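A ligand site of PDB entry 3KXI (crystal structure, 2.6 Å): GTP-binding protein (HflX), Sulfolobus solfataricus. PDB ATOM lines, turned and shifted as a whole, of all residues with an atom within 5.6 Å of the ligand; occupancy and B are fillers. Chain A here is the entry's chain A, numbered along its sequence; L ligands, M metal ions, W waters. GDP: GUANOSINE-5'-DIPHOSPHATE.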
ATOM      1  N   GLU A  14      22.458 -28.672  -2.840  1.00  0.00           N
ATOM      2  CA  GLU A  14      22.844 -27.284  -2.672  1.00  0.00           C
ATOM      3  C   GLU A  14      23.237 -26.730  -4.033  1.00  0.00           C
ATOM      4  O   GLU A  14      23.205 -25.520  -4.263  1.00  0.00           O
ATOM      5  CB  GLU A  14      23.979 -27.127  -1.659  1.00  0.00           C
ATOM      6  CG  GLU A  14      23.944 -25.791  -0.920  1.00  0.00           C
ATOM      7  CD  GLU A  14      25.181 -25.524  -0.076  1.00  0.00           C
ATOM      8  OE1 GLU A  14      25.883 -26.498   0.269  1.00  0.00           O
ATOM      9  OE2 GLU A  14      25.449 -24.339   0.232  1.00  0.00           O
ATOM     10  N   ALA A  18      21.005 -23.336  -5.774  1.00  0.00           N
ATOM     11  CA  ALA A  18      21.717 -22.168  -6.272  1.00  0.00           C
ATOM     12  C   ALA A  18      21.347 -21.894  -7.721  1.00  0.00           C
ATOM     13  O   ALA A  18      21.131 -20.749  -8.126  1.00  0.00           O
ATOM     14  CB  ALA A  18      23.207 -22.353  -6.128  1.00  0.00           C
ATOM     15  N   LEU A  19      21.267 -22.965  -8.503  1.00  0.00           N
ATOM     16  CA  LEU A  19      20.968 -22.869  -9.929  1.00  0.00           C
ATOM     17  C   LEU A  19      19.525 -22.437 -10.180  1.00  0.00           C
ATOM     18  O   LEU A  19      19.256 -21.648 -11.086  1.00  0.00           O
ATOM     19  CB  LEU A  19      21.248 -24.196 -10.624  1.00  0.00           C
ATOM     20  CG  LEU A  19      22.734 -24.435 -10.889  1.00  0.00           C
ATOM     21  CD1 LEU A  19      22.962 -25.819 -11.471  1.00  0.00           C
ATOM     22  CD2 LEU A  19      23.279 -23.356 -11.797  1.00  0.00           C
ATOM     23  N   GLU A  21      17.584 -20.709  -8.138  1.00  0.00           N
ATOM     24  CA  GLU A  21      17.435 -19.312  -7.777  1.00  0.00           C
ATOM     25  C   GLU A  21      18.146 -18.438  -8.799  1.00  0.00           C
ATOM     26  O   GLU A  21      17.728 -17.311  -9.070  1.00  0.00           O
ATOM     27  CB  GLU A  21      17.986 -19.051  -6.374  1.00  0.00           C
ATOM     28  CG  GLU A  21      17.417 -19.977  -5.325  1.00  0.00           C
ATOM     29  CD  GLU A  21      17.704 -19.491  -3.925  1.00  0.00           C
ATOM     30  OE1 GLU A  21      18.219 -18.369  -3.787  1.00  0.00           O
ATOM     31  OE2 GLU A  21      17.413 -20.246  -2.967  1.00  0.00           O
ATOM     32  N   GLY A 186      32.787 -17.404 -11.099  1.00  0.00           N
ATOM     33  CA  GLY A 186      32.970 -18.457 -10.114  1.00  0.00           C
ATOM     34  C   GLY A 186      31.941 -19.571 -10.242  1.00  0.00           C
ATOM     35  O   GLY A 186      30.898 -19.403 -10.881  1.00  0.00           O
ATOM     36  N   TYR A 187      32.246 -20.702  -9.622  1.00  0.00           N
ATOM     37  CA  TYR A 187      31.347 -21.854  -9.660  1.00  0.00           C
ATOM     38  C   TYR A 187      30.022 -21.567  -8.983  1.00  0.00           C
ATOM     39  O   TYR A 187      29.899 -20.634  -8.198  1.00  0.00           O
ATOM     40  CB  TYR A 187      32.006 -23.097  -9.073  1.00  0.00           C
ATOM     41  CG  TYR A 187      32.860 -23.841 -10.078  1.00  0.00           C
ATOM     42  CD1 TYR A 187      34.238 -23.657 -10.110  1.00  0.00           C
ATOM     43  CD2 TYR A 187      32.282 -24.716 -10.987  1.00  0.00           C
ATOM     44  CE1 TYR A 187      35.019 -24.327 -11.037  1.00  0.00           C
ATOM     45  CE2 TYR A 187      33.054 -25.397 -11.910  1.00  0.00           C
ATOM     46  CZ  TYR A 187      34.427 -25.195 -11.929  1.00  0.00           C
ATOM     47  OH  TYR A 187      35.192 -25.877 -12.846  1.00  0.00           O
ATOM     48  N   THR A 188      29.026 -22.385  -9.301  1.00  0.00           N
ATOM     49  CA  THR A 188      27.717 -22.212  -8.709  1.00  0.00           C
ATOM     50  C   THR A 188      27.791 -22.551  -7.233  1.00  0.00           C
ATOM     51  O   THR A 188      28.509 -23.470  -6.834  1.00  0.00           O
ATOM     52  CB  THR A 188      26.649 -23.067  -9.419  1.00  0.00           C
ATOM     53  OG1 THR A 188      27.211 -24.345  -9.733  1.00  0.00           O
ATOM     54  CG2 THR A 188      26.229 -22.396 -10.721  1.00  0.00           C
ATOM     55  N   ASN A 189      27.060 -21.786  -6.431  1.00  0.00           N
ATOM     56  CA  ASN A 189      27.079 -21.936  -4.990  1.00  0.00           C
ATOM     57  C   ASN A 189      28.370 -21.420  -4.364  1.00  0.00           C
ATOM     58  O   ASN A 189      28.597 -21.605  -3.161  1.00  0.00           O
ATOM     59  CB  ASN A 189      26.827 -23.392  -4.595  1.00  0.00           C
ATOM     60  CG  ASN A 189      26.515 -23.548  -3.126  1.00  0.00           C
ATOM     61  OD1 ASN A 189      25.492 -23.071  -2.644  1.00  0.00           O
ATOM     62  ND2 ASN A 189      27.404 -24.222  -2.410  1.00  0.00           N
ATOM     63  N   SER A 190      29.224 -20.777  -5.160  1.00  0.00           N
ATOM     64  CA  SER A 190      30.446 -20.164  -4.642  1.00  0.00           C
ATOM     65  C   SER A 190      30.132 -18.822  -3.980  1.00  0.00           C
ATOM     66  O   SER A 190      30.878 -18.362  -3.122  1.00  0.00           O
ATOM     67  CB  SER A 190      31.472 -19.947  -5.765  1.00  0.00           C
ATOM     68  OG  SER A 190      31.177 -18.794  -6.533  1.00  0.00           O
ATOM     69  N   GLY A 191      29.034 -18.205  -4.398  1.00  0.00           N
ATOM     70  CA  GLY A 191      28.577 -16.949  -3.827  1.00  0.00           C
ATOM     71  C   GLY A 191      28.534 -15.782  -4.809  1.00  0.00           C
ATOM     72  O   GLY A 191      28.439 -14.628  -4.378  1.00  0.00           O
ATOM     73  N   LYS A 192      28.609 -16.074  -6.105  1.00  0.00           N
ATOM     74  CA  LYS A 192      28.589 -15.028  -7.122  1.00  0.00           C
ATOM     75  C   LYS A 192      27.463 -14.038  -6.875  1.00  0.00           C
ATOM     76  O   LYS A 192      27.697 -12.834  -6.748  1.00  0.00           O
ATOM     77  CB  LYS A 192      28.395 -15.603  -8.522  1.00  0.00           C
ATOM     78  CG  LYS A 192      29.615 -16.227  -9.151  1.00  0.00           C
ATOM     79  CD  LYS A 192      29.270 -16.713 -10.553  1.00  0.00           C
ATOM     80  CE  LYS A 192      27.964 -17.509 -10.568  1.00  0.00           C
ATOM     81  NZ  LYS A 192      27.987 -18.787  -9.798  1.00  0.00           N
ATOM     82  N   THR A 193      26.252 -14.562  -6.827  1.00  0.00           N
ATOM     83  CA  THR A 193      25.069 -13.742  -6.649  1.00  0.00           C
ATOM     84  C   THR A 193      25.118 -13.007  -5.310  1.00  0.00           C
ATOM     85  O   THR A 193      24.981 -11.790  -5.269  1.00  0.00           O
ATOM     86  CB  THR A 193      23.766 -14.564  -6.753  1.00  0.00           C
ATOM     87  OG1 THR A 193      23.664 -15.143  -8.054  1.00  0.00           O
ATOM     88  CG2 THR A 193      22.558 -13.682  -6.491  1.00  0.00           C
ATOM     89  N   SER A 194      25.309 -13.751  -4.232  1.00  0.00           N
ATOM     90  CA  SER A 194      25.380 -13.144  -2.902  1.00  0.00           C
ATOM     91  C   SER A 194      26.282 -11.921  -2.923  1.00  0.00           C
ATOM     92  O   SER A 194      25.956 -10.871  -2.372  1.00  0.00           O
ATOM     93  CB  SER A 194      25.864 -14.151  -1.852  1.00  0.00           C
ATOM     94  OG  SER A 194      25.019 -15.285  -1.771  1.00  0.00           O
ATOM     95  N   LEU A 195      27.440 -12.052  -3.569  1.00  0.00           N
ATOM     96  CA  LEU A 195      28.400 -10.961  -3.606  1.00  0.00           C
ATOM     97  C   LEU A 195      27.888  -9.777  -4.426  1.00  0.00           C
ATOM     98  O   LEU A 195      27.905  -8.643  -3.953  1.00  0.00           O
ATOM     99  CB  LEU A 195      29.743 -11.448  -4.158  1.00  0.00           C
ATOM    100  CG  LEU A 195      30.804 -10.356  -4.146  1.00  0.00           C
ATOM    101  CD1 LEU A 195      30.927  -9.783  -2.735  1.00  0.00           C
ATOM    102  CD2 LEU A 195      32.142 -10.879  -4.650  1.00  0.00           C
ATOM    103  N   ASP A 232      26.603  -9.681 -12.493  1.00  0.00           N
ATOM    104  CA  ASP A 232      26.502 -11.052 -12.044  1.00  0.00           C
ATOM    105  C   ASP A 232      26.525 -11.921 -13.294  1.00  0.00           C
ATOM    106  O   ASP A 232      25.578 -11.944 -14.089  1.00  0.00           O
ATOM    107  CB  ASP A 232      25.224 -11.309 -11.240  1.00  0.00           C
ATOM    108  CG  ASP A 232      25.203 -12.716 -10.650  1.00  0.00           C
ATOM    109  OD1 ASP A 232      26.297 -13.267 -10.375  1.00  0.00           O
ATOM    110  OD2 ASP A 232      24.096 -13.271 -10.452  1.00  0.00           O
ATOM    111  N   ASN A 300      35.510 -16.680  -0.477  1.00  0.00           N
ATOM    112  CA  ASN A 300      34.233 -16.359   0.169  1.00  0.00           C
ATOM    113  C   ASN A 300      33.725 -17.472   1.098  1.00  0.00           C
ATOM    114  O   ASN A 300      34.098 -18.646   0.962  1.00  0.00           O
ATOM    115  CB  ASN A 300      33.186 -16.066  -0.913  1.00  0.00           C
ATOM    116  CG  ASN A 300      31.836 -15.710  -0.341  1.00  0.00           C
ATOM    117  OD1 ASN A 300      31.738 -14.938   0.610  1.00  0.00           O
ATOM    118  ND2 ASN A 300      30.776 -16.255  -0.928  1.00  0.00           N
ATOM    119  N   LYS A 301      32.863 -17.077   2.036  1.00  0.00           N
ATOM    120  CA  LYS A 301      32.211 -17.980   2.985  1.00  0.00           C
ATOM    121  C   LYS A 301      33.061 -18.253   4.241  1.00  0.00           C
ATOM    122  O   LYS A 301      32.918 -19.272   4.912  1.00  0.00           O
ATOM    123  CB  LYS A 301      31.777 -19.293   2.321  1.00  0.00           C
ATOM    124  CG  LYS A 301      30.646 -19.123   1.309  1.00  0.00           C
ATOM    125  CD  LYS A 301      30.115 -20.465   0.861  1.00  0.00           C
ATOM    126  CE  LYS A 301      29.119 -20.343  -0.277  1.00  0.00           C
ATOM    127  NZ  LYS A 301      28.590 -21.681  -0.635  1.00  0.00           N
ATOM    128  N   ILE A 302      33.936 -17.296   4.552  1.00  0.00           N
ATOM    129  CA  ILE A 302      34.867 -17.421   5.664  1.00  0.00           C
ATOM    130  C   ILE A 302      34.173 -17.411   7.040  1.00  0.00           C
ATOM    131  O   ILE A 302      34.790 -17.741   8.055  1.00  0.00           O
ATOM    132  CB  ILE A 302      35.963 -16.332   5.595  1.00  0.00           C
ATOM    133  CG1 ILE A 302      35.370 -14.930   5.834  1.00  0.00           C
ATOM    134  CG2 ILE A 302      36.691 -16.394   4.264  1.00  0.00           C
ATOM    135  CD1 ILE A 302      36.424 -13.844   6.074  1.00  0.00           C
ATOM    136  N   ASP A 303      32.896 -17.071   7.070  1.00  0.00           N
ATOM    137  CA  ASP A 303      32.137 -17.105   8.312  1.00  0.00           C
ATOM    138  C   ASP A 303      31.859 -18.551   8.724  1.00  0.00           C
ATOM    139  O   ASP A 303      31.469 -18.825   9.858  1.00  0.00           O
ATOM    140  CB  ASP A 303      30.812 -16.355   8.139  1.00  0.00           C
ATOM    141  CG  ASP A 303      30.001 -16.893   6.981  1.00  0.00           C
ATOM    142  OD1 ASP A 303      30.409 -16.686   5.812  1.00  0.00           O
ATOM    143  OD2 ASP A 303      28.960 -17.525   7.255  1.00  0.00           O
ATOM    144  N   LYS A 304      32.068 -19.473   7.784  1.00  0.00           N
ATOM    145  CA  LYS A 304      32.002 -20.890   8.088  1.00  0.00           C
ATOM    146  C   LYS A 304      33.392 -21.338   8.488  1.00  0.00           C
ATOM    147  O   LYS A 304      34.039 -22.138   7.811  1.00  0.00           O
ATOM    148  CB  LYS A 304      31.491 -21.698   6.892  1.00  0.00           C
ATOM    149  N   ILE A 333      36.758 -13.173   2.226  1.00  0.00           N
ATOM    150  CA  ILE A 333      35.521 -12.423   2.381  1.00  0.00           C
ATOM    151  C   ILE A 333      34.371 -13.289   2.891  1.00  0.00           C
ATOM    152  O   ILE A 333      34.455 -14.522   2.894  1.00  0.00           O
ATOM    153  CB  ILE A 333      35.103 -11.738   1.068  1.00  0.00           C
ATOM    154  CG1 ILE A 333      34.835 -12.771  -0.044  1.00  0.00           C
ATOM    155  CG2 ILE A 333      36.148 -10.727   0.627  1.00  0.00           C
ATOM    156  CD1 ILE A 333      33.722 -12.366  -1.006  1.00  0.00           C
ATOM    157  N   SER A 334      33.306 -12.630   3.322  1.00  0.00           N
ATOM    158  CA  SER A 334      32.048 -13.315   3.608  1.00  0.00           C
ATOM    159  C   SER A 334      30.890 -12.497   3.019  1.00  0.00           C
ATOM    160  O   SER A 334      30.391 -11.585   3.662  1.00  0.00           O
ATOM    161  CB  SER A 334      31.855 -13.491   5.113  1.00  0.00           C
ATOM    162  OG  SER A 334      30.581 -14.056   5.397  1.00  0.00           O
ATOM    163  N   ALA A 335      30.498 -12.839   1.790  1.00  0.00           N
ATOM    164  CA  ALA A 335      29.420 -12.139   1.095  1.00  0.00           C
ATOM    165  C   ALA A 335      28.152 -12.117   1.947  1.00  0.00           C
ATOM    166  O   ALA A 335      27.419 -11.127   1.983  1.00  0.00           O
ATOM    167  CB  ALA A 335      29.134 -12.791  -0.250  1.00  0.00           C
ATOM    168  N   LEU A 336      27.917 -13.223   2.640  1.00  0.00           N
ATOM    169  CA  LEU A 336      26.772 -13.369   3.528  1.00  0.00           C
ATOM    170  C   LEU A 336      26.853 -12.386   4.698  1.00  0.00           C
ATOM    171  O   LEU A 336      25.995 -11.507   4.850  1.00  0.00           O
ATOM    172  CB  LEU A 336      26.701 -14.820   4.013  1.00  0.00           C
ATOM    173  CG  LEU A 336      25.439 -15.409   4.646  1.00  0.00           C
ATOM    174  CD1 LEU A 336      25.558 -15.385   6.158  1.00  0.00           C
ATOM    175  CD2 LEU A 336      24.163 -14.701   4.166  1.00  0.00           C
ATOM    176  N   LYS A 337      27.913 -12.500   5.494  1.00  0.00           N
ATOM    177  CA  LYS A 337      28.090 -11.681   6.701  1.00  0.00           C
ATOM    178  C   LYS A 337      28.704 -10.287   6.451  1.00  0.00           C
ATOM    179  O   LYS A 337      28.732  -9.447   7.355  1.00  0.00           O
ATOM    180  CB  LYS A 337      28.921 -12.452   7.726  1.00  0.00           C
ATOM    181  CG  LYS A 337      28.270 -13.727   8.230  1.00  0.00           C
ATOM    182  CD  LYS A 337      27.401 -13.471   9.451  1.00  0.00           C
ATOM    183  CE  LYS A 337      26.021 -14.146   9.358  1.00  0.00           C
ATOM    184  NZ  LYS A 337      25.088 -13.391   8.471  1.00  0.00           N
HETATM  185  PB  GDP L   1      26.380 -18.587  -6.757  1.00  0.00           P
HETATM  186  O1B GDP L   1      25.650 -19.738  -7.408  1.00  0.00           O
HETATM  187  O2B GDP L   1      27.858 -18.701  -7.044  1.00  0.00           O
HETATM  188  O3B GDP L   1      25.898 -17.272  -7.294  1.00  0.00           O
HETATM  189  O3A GDP L   1      26.141 -18.653  -5.170  1.00  0.00           O
HETATM  190  PA  GDP L   1      24.896 -17.965  -4.428  1.00  0.00           P
HETATM  191  O1A GDP L   1      25.043 -16.457  -4.383  1.00  0.00           O
HETATM  192  O2A GDP L   1      23.600 -18.374  -5.088  1.00  0.00           O
HETATM  193  O5' GDP L   1      25.051 -18.590  -2.960  1.00  0.00           O
HETATM  194  C5' GDP L   1      25.110 -20.025  -2.804  1.00  0.00           C
HETATM  195  C4' GDP L   1      24.731 -20.329  -1.368  1.00  0.00           C
HETATM  196  O4' GDP L   1      25.819 -20.013  -0.501  1.00  0.00           O
HETATM  197  C3' GDP L   1      23.595 -19.400  -1.021  1.00  0.00           C
HETATM  198  O3' GDP L   1      22.515 -20.148  -0.451  1.00  0.00           O
HETATM  199  C2' GDP L   1      24.171 -18.413  -0.028  1.00  0.00           C
HETATM  200  O2' GDP L   1      23.233 -18.134   1.019  1.00  0.00           O
HETATM  201  C1' GDP L   1      25.416 -19.092   0.511  1.00  0.00           C
HETATM  202  N9  GDP L   1      26.493 -18.085   0.720  1.00  0.00           N
HETATM  203  C8  GDP L   1      26.920 -17.198  -0.192  1.00  0.00           C
HETATM  204  N7  GDP L   1      27.910 -16.423   0.306  1.00  0.00           N
HETATM  205  C5  GDP L   1      28.150 -16.830   1.569  1.00  0.00           C
HETATM  206  C6  GDP L   1      29.078 -16.449   2.655  1.00  0.00           C
HETATM  207  O6  GDP L   1      29.903 -15.524   2.511  1.00  0.00           O
HETATM  208  N1  GDP L   1      28.992 -17.139   3.811  1.00  0.00           N
HETATM  209  C2  GDP L   1      28.105 -18.140   3.996  1.00  0.00           C
HETATM  210  N2  GDP L   1      28.085 -18.778   5.186  1.00  0.00           N
HETATM  211  N3  GDP L   1      27.234 -18.529   3.043  1.00  0.00           N
HETATM  212  C4  GDP L   1      27.211 -17.931   1.832  1.00  0.00           C
HETATM  213 MG    MG M   1      23.760 -17.484  -9.417  1.00  0.00          MG
HETATM  214  O   HOH W   1      22.234 -18.548  -7.439  1.00  0.00           O
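The backbone NH of Leu 336 sits at hydrogen-bond distance from an oxygen (O6) of the ligand (3.0 Å). An oxygen (O4') of the ligand lies within hydrogen-bond range of the side-chain amino group (NZ) of Lys 301 (3.2 Å). OD1 of Asp 303 sits at hydrogen-bond distance from N1 of the ligand (2.5 Å). The side-chain hydroxyl (OG) of Ser 334 sits close to an oxygen (O6) of the ligand, 3.3 Å away. The side-chain hydroxyl (OG) of Ser 194 lies within hydrogen-bond range of an oxygen (O1A) of the ligand (2.9 Å). N of Ser 190 sits at hydrogen-bond distance from O2B of the ligand (3.1 Å). An oxygen (O6) of the ligand sits at hydrogen-bond distance from the backbone NH of Ala 335 (2.8 Å). An oxygen (O2B) of the ligand lies close to the backbone carbonyl oxygen (O) of Tyr 187. The backbone NH of Thr 193 sits at hydrogen-bond distance from an oxygen (O3B) of the ligand (2.8 Å). An oxygen (O3B) of the ligand lies within hydrogen-bond range of the side-chain hydroxyl (OG1) of Thr 193 (3.2 Å). The backbone NH (N) of Ser 194 sits at hydrogen-bond distance from an oxygen (O1A) of the ligand, at 2.7 Å. OG of Ser 190 is in hydrogen-bond range of O2B of the ligand, at 3.4 Å. N of Gly 191 lies within hydrogen-bond range of O2B of the ligand (2.9 Å). The side-chain amino group (NZ) of Lys 192 is in salt-bridge range of an oxygen (O2B) of the ligand. O6 of the ligand sits at hydrogen-bond distance from N of Lys 301. The side-chain amide oxygen (OD1) of Asn 300 lies close to an oxygen (O6) of the ligand. N of Asn 189 sits at hydrogen-bond distance from O1B of the ligand (2.7 Å). The backbone NH (N) of Lys 192 sits at hydrogen-bond distance from an oxygen (O2B) of the ligand (2.9 Å).
OD1 of Asn 189 sits close to OE2 of Glu 14, at 3.1 Å. The backbone NH (N) of Lys 301 lies within hydrogen-bond range of the backbone carbonyl oxygen (O) of Ile 333 (3.1 Å). NZ of Lys 301 lies within hydrogen-bond range of O of Asn 189 (2.5 Å). The side-chain hydroxyl (OG) of Ser 190 sits at hydrogen-bond distance from the backbone carbonyl oxygen (O) of Tyr 187 (2.8 Å). OD2 of Asp 232 lies within hydrogen-bond range of OG1 of Thr 193 (3.1 Å). OG of Ser 334 lies within hydrogen-bond range of N of Lys 337 (3.1 Å). The side-chain carboxylate (OD1) of Asp 303 sits at hydrogen-bond distance from the side-chain hydroxyl (OG) of Ser 334 (2.7 Å). The backbone carbonyl oxygen (O) of Tyr 187 is in hydrogen-bond range of the side-chain amino group (NZ) of Lys 192, at 3.1 Å.
CB of Ala 18 touches O1B of the ligand (3.8 Å). Thr 188 touches the ligand. Hydrophobic or aromatic side chains within 4 Å of the ligand: Ala 18, Ala 335 and Leu 336. Of the 25 residues printed, 15 come within 4 Å of the ligand. The nearest printed residue that does not touch the ligand is Glu 14 (4.4 Å).
Water W1 bridges O of Ala 18 (2.6 Å) and O2A of the ligand (2.7 Å).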
